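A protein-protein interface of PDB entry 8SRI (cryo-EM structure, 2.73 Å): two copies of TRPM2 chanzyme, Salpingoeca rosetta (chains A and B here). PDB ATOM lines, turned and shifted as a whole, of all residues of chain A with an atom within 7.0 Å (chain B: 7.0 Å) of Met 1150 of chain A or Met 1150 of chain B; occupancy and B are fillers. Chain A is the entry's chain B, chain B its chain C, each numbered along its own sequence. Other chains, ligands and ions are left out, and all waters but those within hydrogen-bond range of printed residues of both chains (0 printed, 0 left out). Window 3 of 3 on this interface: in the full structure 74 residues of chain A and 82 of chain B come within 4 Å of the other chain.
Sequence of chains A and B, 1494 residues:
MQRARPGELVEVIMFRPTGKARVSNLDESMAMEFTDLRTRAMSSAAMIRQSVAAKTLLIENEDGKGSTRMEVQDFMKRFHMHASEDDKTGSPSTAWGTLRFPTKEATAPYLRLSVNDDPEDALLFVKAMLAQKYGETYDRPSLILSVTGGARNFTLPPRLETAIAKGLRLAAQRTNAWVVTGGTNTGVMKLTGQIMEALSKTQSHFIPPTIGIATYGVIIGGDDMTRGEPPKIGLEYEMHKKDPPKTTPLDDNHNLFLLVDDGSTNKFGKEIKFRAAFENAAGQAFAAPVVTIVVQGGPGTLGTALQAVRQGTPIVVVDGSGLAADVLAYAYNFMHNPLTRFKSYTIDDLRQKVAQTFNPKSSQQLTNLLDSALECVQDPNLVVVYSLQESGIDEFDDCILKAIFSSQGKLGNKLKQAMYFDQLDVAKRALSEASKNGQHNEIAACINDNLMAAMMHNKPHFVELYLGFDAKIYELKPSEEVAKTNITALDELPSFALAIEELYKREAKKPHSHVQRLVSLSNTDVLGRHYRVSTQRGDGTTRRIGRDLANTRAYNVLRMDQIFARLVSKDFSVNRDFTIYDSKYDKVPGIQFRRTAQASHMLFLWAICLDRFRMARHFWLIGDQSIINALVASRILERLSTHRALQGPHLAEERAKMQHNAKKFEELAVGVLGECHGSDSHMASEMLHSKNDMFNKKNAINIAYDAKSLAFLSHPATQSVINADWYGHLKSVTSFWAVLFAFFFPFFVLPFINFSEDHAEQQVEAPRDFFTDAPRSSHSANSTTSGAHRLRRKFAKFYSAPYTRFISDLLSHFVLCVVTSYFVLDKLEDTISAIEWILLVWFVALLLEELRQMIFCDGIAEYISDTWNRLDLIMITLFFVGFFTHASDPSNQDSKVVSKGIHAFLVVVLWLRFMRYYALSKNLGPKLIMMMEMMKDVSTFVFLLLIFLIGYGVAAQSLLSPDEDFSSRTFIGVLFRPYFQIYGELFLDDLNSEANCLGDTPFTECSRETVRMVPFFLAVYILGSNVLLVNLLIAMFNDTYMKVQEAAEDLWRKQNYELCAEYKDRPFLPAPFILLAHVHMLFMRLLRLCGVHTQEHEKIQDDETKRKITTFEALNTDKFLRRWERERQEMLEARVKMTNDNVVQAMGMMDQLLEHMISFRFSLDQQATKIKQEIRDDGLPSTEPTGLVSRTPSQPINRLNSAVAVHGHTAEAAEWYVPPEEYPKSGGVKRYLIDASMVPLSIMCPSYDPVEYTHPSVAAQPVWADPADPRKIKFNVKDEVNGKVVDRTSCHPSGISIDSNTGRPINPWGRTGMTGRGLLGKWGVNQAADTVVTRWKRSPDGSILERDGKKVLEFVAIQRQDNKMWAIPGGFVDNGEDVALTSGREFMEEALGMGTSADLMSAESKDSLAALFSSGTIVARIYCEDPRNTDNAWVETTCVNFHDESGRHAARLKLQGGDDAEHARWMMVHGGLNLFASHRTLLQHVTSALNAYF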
ATOM      1  N   GLN A1145      18.342   7.082   2.354  1.00  0.00           N
ATOM      2  CA  GLN A1145      18.044   8.520   2.229  1.00  0.00           C
ATOM      3  C   GLN A1145      18.074   9.009   0.774  1.00  0.00           C
ATOM      4  O   GLN A1145      17.301   9.906   0.411  1.00  0.00           O
ATOM      5  CB  GLN A1145      19.001   9.359   3.080  1.00  0.00           C
ATOM      6  CG  GLN A1145      18.868   9.165   4.584  1.00  0.00           C
ATOM      7  CD  GLN A1145      19.862  10.004   5.366  1.00  0.00           C
ATOM      8  OE1 GLN A1145      20.588  10.818   4.796  1.00  0.00           O
ATOM      9  NE2 GLN A1145      19.897   9.810   6.680  1.00  0.00           N
ATOM     10  N   ALA A1146      18.962   8.413  -0.046  1.00  0.00           N
ATOM     11  CA  ALA A1146      19.059   8.666  -1.486  1.00  0.00           C
ATOM     12  C   ALA A1146      17.787   8.247  -2.232  1.00  0.00           C
ATOM     13  O   ALA A1146      17.352   8.951  -3.161  1.00  0.00           O
ATOM     14  CB  ALA A1146      20.301   7.961  -2.033  1.00  0.00           C
ATOM     15  N   MET A1147      17.226   7.068  -1.867  1.00  0.00           N
ATOM     16  CA  MET A1147      15.924   6.601  -2.376  1.00  0.00           C
ATOM     17  C   MET A1147      14.789   7.551  -1.990  1.00  0.00           C
ATOM     18  O   MET A1147      13.845   7.733  -2.782  1.00  0.00           O
ATOM     19  CB  MET A1147      15.611   5.185  -1.886  1.00  0.00           C
ATOM     20  CG  MET A1147      16.485   4.084  -2.458  1.00  0.00           C
ATOM     21  SD  MET A1147      16.044   2.461  -1.805  1.00  0.00           S
ATOM     22  CE  MET A1147      14.417   2.233  -2.511  1.00  0.00           C
ATOM     23  N   GLY A1148      14.830   8.057  -0.733  1.00  0.00           N
ATOM     24  CA  GLY A1148      13.869   9.063  -0.249  1.00  0.00           C
ATOM     25  C   GLY A1148      13.891  10.352  -1.066  1.00  0.00           C
ATOM     26  O   GLY A1148      12.829  10.920  -1.391  1.00  0.00           O
ATOM     27  N   MET A1149      15.114  10.830  -1.382  1.00  0.00           N
ATOM     28  CA  MET A1149      15.310  12.026  -2.208  1.00  0.00           C
ATOM     29  C   MET A1149      14.845  11.798  -3.648  1.00  0.00           C
ATOM     30  O   MET A1149      14.332  12.736  -4.267  1.00  0.00           O
ATOM     31  CB  MET A1149      16.764  12.505  -2.162  1.00  0.00           C
ATOM     32  CG  MET A1149      17.190  13.033  -0.799  1.00  0.00           C
ATOM     33  SD  MET A1149      18.916  13.530  -0.703  1.00  0.00           S
ATOM     34  CE  MET A1149      19.393  12.687   0.802  1.00  0.00           C
ATOM     35  N   MET A1150      15.039  10.570  -4.189  1.00  0.00           N
ATOM     36  CA  MET A1150      14.493  10.207  -5.512  1.00  0.00           C
ATOM     37  C   MET A1150      12.969  10.198  -5.544  1.00  0.00           C
ATOM     38  O   MET A1150      12.388  10.457  -6.609  1.00  0.00           O
ATOM     39  CB  MET A1150      14.995   8.873  -6.044  1.00  0.00           C
ATOM     40  CG  MET A1150      16.417   8.832  -6.419  1.00  0.00           C
ATOM     41  SD  MET A1150      16.718   7.176  -7.008  1.00  0.00           S
ATOM     42  CE  MET A1150      18.441   7.355  -7.308  1.00  0.00           C
ATOM     43  N   ASP A1151      12.332   9.750  -4.438  1.00  0.00           N
ATOM     44  CA  ASP A1151      10.868   9.797  -4.294  1.00  0.00           C
ATOM     45  C   ASP A1151      10.365  11.243  -4.349  1.00  0.00           C
ATOM     46  O   ASP A1151       9.323  11.517  -4.976  1.00  0.00           O
ATOM     47  CB  ASP A1151      10.415   9.110  -3.005  1.00  0.00           C
ATOM     48  CG  ASP A1151      10.604   7.602  -3.043  1.00  0.00           C
ATOM     49  OD1 ASP A1151      10.253   6.985  -4.071  1.00  0.00           O
ATOM     50  OD2 ASP A1151      11.047   7.025  -2.028  1.00  0.00           O
ATOM     51  N   GLN A1152      11.089  12.153  -3.654  1.00  0.00           N
ATOM     52  CA  GLN A1152      10.824  13.601  -3.698  1.00  0.00           C
ATOM     53  C   GLN A1152      10.997  14.171  -5.121  1.00  0.00           C
ATOM     54  O   GLN A1152      10.186  15.014  -5.552  1.00  0.00           O
ATOM     55  CB  GLN A1152      11.737  14.328  -2.706  1.00  0.00           C
ATOM     56  CG  GLN A1152      11.406  15.805  -2.487  1.00  0.00           C
ATOM     57  CD  GLN A1152      11.791  16.296  -1.101  1.00  0.00           C
ATOM     58  OE1 GLN A1152      11.105  17.131  -0.509  1.00  0.00           O
ATOM     59  NE2 GLN A1152      12.898  15.781  -0.578  1.00  0.00           N
ATOM     60  N   LEU A1153      12.074  13.738  -5.832  1.00  0.00           N
ATOM     61  CA  LEU A1153      12.359  14.134  -7.227  1.00  0.00           C
ATOM     62  C   LEU A1153      11.254  13.688  -8.186  1.00  0.00           C
ATOM     63  O   LEU A1153      10.858  14.460  -9.067  1.00  0.00           O
ATOM     64  CB  LEU A1153      13.706  13.601  -7.733  1.00  0.00           C
ATOM     65  CG  LEU A1153      15.091  14.080  -7.269  1.00  0.00           C
ATOM     66  CD1 LEU A1153      16.176  13.117  -7.745  1.00  0.00           C
ATOM     67  CD2 LEU A1153      15.400  15.506  -7.698  1.00  0.00           C
ATOM     68  N   LEU A1154      10.762  12.439  -8.014  1.00  0.00           N
ATOM     69  CA  LEU A1154       9.698  11.855  -8.842  1.00  0.00           C
ATOM     70  C   LEU A1154       8.371  12.575  -8.619  1.00  0.00           C
ATOM     71  O   LEU A1154       7.564  12.694  -9.558  1.00  0.00           O
ATOM     72  CB  LEU A1154       9.556  10.359  -8.560  1.00  0.00           C
ATOM     73  CG  LEU A1154      10.543   9.467  -9.313  1.00  0.00           C
ATOM     74  CD1 LEU A1154      10.491   8.040  -8.798  1.00  0.00           C
ATOM     75  CD2 LEU A1154      10.265   9.516 -10.808  1.00  0.00           C
ATOM     76  N   GLU A1155       8.130  12.990  -7.356  1.00  0.00           N
ATOM     77  CA  GLU A1155       6.983  13.823  -6.977  1.00  0.00           C
ATOM     78  C   GLU A1155       7.020  15.171  -7.702  1.00  0.00           C
ATOM     79  O   GLU A1155       5.975  15.644  -8.190  1.00  0.00           O
ATOM     80  CB  GLU A1155       6.967  13.980  -5.452  1.00  0.00           C
ATOM     81  CG  GLU A1155       6.319  15.228  -4.856  1.00  0.00           C
ATOM     82  CD  GLU A1155       4.821  15.289  -5.032  1.00  0.00           C
ATOM     83  OE1 GLU A1155       4.171  14.224  -5.091  1.00  0.00           O
ATOM     84  OE2 GLU A1155       4.285  16.418  -5.044  1.00  0.00           O
ATOM     85  N   HIS A1156       8.220  15.795  -7.758  1.00  0.00           N
ATOM     86  CA  HIS A1156       8.419  17.053  -8.493  1.00  0.00           C
ATOM     87  C   HIS A1156       8.216  16.887 -10.010  1.00  0.00           C
ATOM     88  O   HIS A1156       7.699  17.811 -10.662  1.00  0.00           O
ATOM     89  CB  HIS A1156       9.796  17.655  -8.202  1.00  0.00           C
ATOM     90  CG  HIS A1156       9.856  18.467  -6.942  1.00  0.00           C
ATOM     91  ND1 HIS A1156       9.383  19.760  -6.877  1.00  0.00           N
ATOM     92  CD2 HIS A1156      10.366  18.193  -5.719  1.00  0.00           C
ATOM     93  CE1 HIS A1156       9.577  20.238  -5.660  1.00  0.00           C
ATOM     94  NE2 HIS A1156      10.171  19.306  -4.937  1.00  0.00           N
ATOM     95  N   ASN B1142      18.764  -2.230  -3.554  1.00  0.00           N
ATOM     96  CA  ASN B1142      18.366  -0.822  -3.430  1.00  0.00           C
ATOM     97  C   ASN B1142      19.000   0.033  -4.535  1.00  0.00           C
ATOM     98  O   ASN B1142      18.349   0.933  -5.078  1.00  0.00           O
ATOM     99  CB  ASN B1142      18.735  -0.280  -2.049  1.00  0.00           C
ATOM    100  CG  ASN B1142      17.778  -0.736  -0.965  1.00  0.00           C
ATOM    101  OD1 ASN B1142      16.651  -1.144  -1.248  1.00  0.00           O
ATOM    102  ND2 ASN B1142      18.217  -0.654   0.285  1.00  0.00           N
ATOM    103  N   VAL B1143      20.280  -0.236  -4.851  1.00  0.00           N
ATOM    104  CA  VAL B1143      21.018   0.459  -5.916  1.00  0.00           C
ATOM    105  C   VAL B1143      20.447   0.102  -7.306  1.00  0.00           C
ATOM    106  O   VAL B1143      20.389   0.968  -8.201  1.00  0.00           O
ATOM    107  CB  VAL B1143      22.535   0.173  -5.727  1.00  0.00           C
ATOM    108  CG1 VAL B1143      23.434   0.433  -6.936  1.00  0.00           C
ATOM    109  CG2 VAL B1143      23.074   1.091  -4.636  1.00  0.00           C
ATOM    110  N   GLN B1145      17.155  -0.790  -7.857  1.00  0.00           N
ATOM    111  CA  GLN B1145      15.900  -0.015  -7.861  1.00  0.00           C
ATOM    112  C   GLN B1145      16.133   1.489  -8.055  1.00  0.00           C
ATOM    113  O   GLN B1145      15.303   2.164  -8.682  1.00  0.00           O
ATOM    114  CB  GLN B1145      15.094  -0.257  -6.582  1.00  0.00           C
ATOM    115  CG  GLN B1145      14.560  -1.673  -6.413  1.00  0.00           C
ATOM    116  CD  GLN B1145      13.795  -1.852  -5.115  1.00  0.00           C
ATOM    117  OE1 GLN B1145      13.567  -0.892  -4.379  1.00  0.00           O
ATOM    118  NE2 GLN B1145      13.393  -3.085  -4.829  1.00  0.00           N
ATOM    119  N   ALA B1146      17.259   2.000  -7.522  1.00  0.00           N
ATOM    120  CA  ALA B1146      17.704   3.386  -7.698  1.00  0.00           C
ATOM    121  C   ALA B1146      18.015   3.709  -9.164  1.00  0.00           C
ATOM    122  O   ALA B1146      17.698   4.816  -9.636  1.00  0.00           O
ATOM    123  CB  ALA B1146      18.908   3.641  -6.788  1.00  0.00           C
ATOM    124  N   MET B1147      18.692   2.768  -9.866  1.00  0.00           N
ATOM    125  CA  MET B1147      18.931   2.859 -11.318  1.00  0.00           C
ATOM    126  C   MET B1147      17.622   2.872 -12.109  1.00  0.00           C
ATOM    127  O   MET B1147      17.539   3.557 -13.146  1.00  0.00           O
ATOM    128  CB  MET B1147      19.828   1.718 -11.807  1.00  0.00           C
ATOM    129  CG  MET B1147      21.270   1.768 -11.337  1.00  0.00           C
ATOM    130  SD  MET B1147      22.231   0.373 -11.954  1.00  0.00           S
ATOM    131  CE  MET B1147      22.258   0.719 -13.709  1.00  0.00           C
ATOM    132  N   GLY B1148      16.652   2.026 -11.681  1.00  0.00           N
ATOM    133  CA  GLY B1148      15.304   1.997 -12.274  1.00  0.00           C
ATOM    134  C   GLY B1148      14.574   3.334 -12.161  1.00  0.00           C
ATOM    135  O   GLY B1148      13.924   3.788 -13.123  1.00  0.00           O
ATOM    136  N   MET B1149      14.665   3.958 -10.967  1.00  0.00           N
ATOM    137  CA  MET B1149      14.069   5.274 -10.711  1.00  0.00           C
ATOM    138  C   MET B1149      14.759   6.372 -11.525  1.00  0.00           C
ATOM    139  O   MET B1149      14.084   7.314 -11.953  1.00  0.00           O
ATOM    140  CB  MET B1149      14.069   5.606  -9.217  1.00  0.00           C
ATOM    141  CG  MET B1149      13.147   4.717  -8.394  1.00  0.00           C
ATOM    142  SD  MET B1149      13.188   5.041  -6.625  1.00  0.00           S
ATOM    143  CE  MET B1149      13.383   3.371  -6.014  1.00  0.00           C
ATOM    144  N   MET B1150      16.097   6.268 -11.723  1.00  0.00           N
ATOM    145  CA  MET B1150      16.826   7.191 -12.615  1.00  0.00           C
ATOM    146  C   MET B1150      16.401   7.067 -14.074  1.00  0.00           C
ATOM    147  O   MET B1150      16.479   8.062 -14.810  1.00  0.00           O
ATOM    148  CB  MET B1150      18.340   7.058 -12.539  1.00  0.00           C
ATOM    149  CG  MET B1150      18.956   7.502 -11.279  1.00  0.00           C
ATOM    150  SD  MET B1150      20.710   7.243 -11.477  1.00  0.00           S
ATOM    151  CE  MET B1150      21.193   7.758  -9.867  1.00  0.00           C
ATOM    152  N   ASP B1151      16.109   5.827 -14.528  1.00  0.00           N
ATOM    153  CA  ASP B1151      15.578   5.581 -15.878  1.00  0.00           C
ATOM    154  C   ASP B1151      14.226   6.279 -16.062  1.00  0.00           C
ATOM    155  O   ASP B1151      13.964   6.857 -17.135  1.00  0.00           O
ATOM    156  CB  ASP B1151      15.461   4.083 -16.166  1.00  0.00           C
ATOM    157  CG  ASP B1151      16.814   3.407 -16.315  1.00  0.00           C
ATOM    158  OD1 ASP B1151      17.687   3.969 -17.010  1.00  0.00           O
ATOM    159  OD2 ASP B1151      16.988   2.288 -15.789  1.00  0.00           O
ATOM    160  N   GLN B1152      13.360   6.185 -15.025  1.00  0.00           N
ATOM    161  CA  GLN B1152      12.071   6.897 -14.977  1.00  0.00           C
ATOM    162  C   GLN B1152      12.262   8.427 -15.012  1.00  0.00           C
ATOM    163  O   GLN B1152      11.498   9.131 -15.699  1.00  0.00           O
ATOM    164  CB  GLN B1152      11.286   6.473 -13.732  1.00  0.00           C
ATOM    165  CG  GLN B1152       9.838   6.964 -13.685  1.00  0.00           C
ATOM    166  CD  GLN B1152       8.925   6.033 -12.903  1.00  0.00           C
ATOM    167  OE1 GLN B1152       7.755   5.855 -13.247  1.00  0.00           O
ATOM    168  NE2 GLN B1152       9.458   5.436 -11.843  1.00  0.00           N
ATOM    169  N   LEU B1153      13.258   8.941 -14.238  1.00  0.00           N
ATOM    170  CA  LEU B1153      13.618  10.373 -14.196  1.00  0.00           C
ATOM    171  C   LEU B1153      14.094  10.886 -15.556  1.00  0.00           C
ATOM    172  O   LEU B1153      13.709  11.987 -15.966  1.00  0.00           O
ATOM    173  CB  LEU B1153      14.687  10.686 -13.140  1.00  0.00           C
ATOM    174  CG  LEU B1153      14.484  10.649 -11.618  1.00  0.00           C
ATOM    175  CD1 LEU B1153      15.828  10.703 -10.897  1.00  0.00           C
ATOM    176  CD2 LEU B1153      13.551  11.741 -11.117  1.00  0.00           C
ATOM    177  N   LEU B1154      14.935  10.085 -16.250  1.00  0.00           N
ATOM    178  CA  LEU B1154      15.483  10.420 -17.571  1.00  0.00           C
ATOM    179  C   LEU B1154      14.385  10.445 -18.630  1.00  0.00           C
ATOM    180  O   LEU B1154      14.460  11.242 -19.583  1.00  0.00           O
ATOM    181  CB  LEU B1154      16.589   9.439 -17.961  1.00  0.00           C
ATOM    182  CG  LEU B1154      17.966   9.759 -17.380  1.00  0.00           C
ATOM    183  CD1 LEU B1154      18.937   8.615 -17.618  1.00  0.00           C
ATOM    184  CD2 LEU B1154      18.499  11.054 -17.969  1.00  0.00           C
ATOM    185  N   GLU B1155      13.407   9.524 -18.490  1.00  0.00           N
ATOM    186  CA  GLU B1155      12.197   9.484 -19.320  1.00  0.00           C
ATOM    187  C   GLU B1155      11.382  10.770 -19.160  1.00  0.00           C
ATOM    188  O   GLU B1155      10.888  11.323 -20.164  1.00  0.00           O
ATOM    189  CB  GLU B1155      11.389   8.233 -18.959  1.00  0.00           C
ATOM    190  CG  GLU B1155       9.878   8.254 -19.176  1.00  0.00           C
ATOM    191  CD  GLU B1155       9.465   8.291 -20.628  1.00  0.00           C
ATOM    192  OE1 GLU B1155      10.205   7.764 -21.485  1.00  0.00           O
ATOM    193  OE2 GLU B1155       8.355   8.795 -20.901  1.00  0.00           O
ATOM    194  N   HIS B1156      11.228  11.237 -17.899  1.00  0.00           N
ATOM    195  CA  HIS B1156      10.540  12.504 -17.607  1.00  0.00           C
ATOM    196  C   HIS B1156      11.287  13.724 -18.175  1.00  0.00           C
ATOM    197  O   HIS B1156      10.638  14.688 -18.617  1.00  0.00           O
ATOM    198  CB  HIS B1156      10.304  12.676 -16.104  1.00  0.00           C
ATOM    199  CG  HIS B1156       9.079  11.977 -15.591  1.00  0.00           C
ATOM    200  ND1 HIS B1156       7.814  12.499 -15.752  1.00  0.00           N
ATOM    201  CD2 HIS B1156       8.924  10.829 -14.891  1.00  0.00           C
ATOM    202  CE1 HIS B1156       6.930  11.691 -15.194  1.00  0.00           C
ATOM    203  NE2 HIS B1156       7.578  10.669 -14.665  1.00  0.00           N
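Of the 12 printed residues of chain A, 4 touch a printed residue of chain B.
Printed residues of chain A that touch a printed residue of chain B: Met 1147, Met 1150, Leu 1153 and Leu 1154.
Printed residues of chain B that touch a printed residue of chain A: Asn 1142, Gln 1145, Ala 1146, Met 1149, Met 1150, Gln 1152 and Leu 1153.
Hydrophobic or aromatic side chains of chain B within 4 Å of the printed part of chain A: Ala 1146, Met 1149, Met 1150 and Leu 1153.
Among the printed residues, merely in contact across the chains: Met 1147 of chain A with Gln 1145 of chain B (3.7 Å), Met 1150 of chain A with Met 1150 of chain B (3.8 Å), Met 1150 of chain A with Met 1149 of chain B (3.8 Å), Met 1147 of chain A with Met 1149 of chain B (3.8 Å), Leu 1153 of chain A with Leu 1153 of chain B (3.9 Å), Leu 1154 of chain A with Gln 1152 of chain B (3.9 Å) and Leu 1154 of chain A with Leu 1153 of chain B (3.98 Å).
Met 1147 of chain A touches Gln 1145 of chain B, but with the chains exchanged Gln 1145 of chain A does not touch Met 1147 of chain B (12.4 Å).
Met 1150 of chain A touches Ala 1146 of chain B, but with the chains exchanged Ala 1146 of chain A does not touch Met 1150 of chain B (7.8 Å).
Met 1150 of chain A touches Met 1149 of chain B, but with the chains exchanged Met 1149 of chain A does not touch Met 1150 of chain B (9.7 Å).
Leu 1153 of chain B touches its own counterpart, Leu 1153 of chain A.
Of the printed residues of chain B, Met 1147 of chain A touches Asn 1142, Gln 1145 and Met 1149.
Met 1150 of chain A touches just these residues of chain B: Ala 1146 (3.5 Å), Met 1149 (3.8 Å) and Met 1150 (3.8 Å).
Of the printed residues of chain A, Ala 1146 of chain B touches Met 1150 (3.5 Å).
Of the printed residues of chain A, Met 1150 of chain B touches Met 1150 (3.8 Å).
Of the printed residues of chain A, Gln 1152 of chain B touches Leu 1154.
The nearest residue of chain B that does not touch Met 1150 of chain A is Leu 1153 of chain B (4.8 Å).
The nearest printed residue of chain A that does not touch Ala 1146 of chain B is Met 1147 of chain A (5.0 Å).
The side-chain sulfur (SD) of Met 1150 of chain A sits close to the backbone carbonyl oxygen (O) of Ala 1146 of chain B (3.7 Å).
The side-chain sulfur (SD) of Met 1147 of chain A lies close to the side-chain amide oxygen (OD1) of Asn 1142 of chain B, at 3.7 Å.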
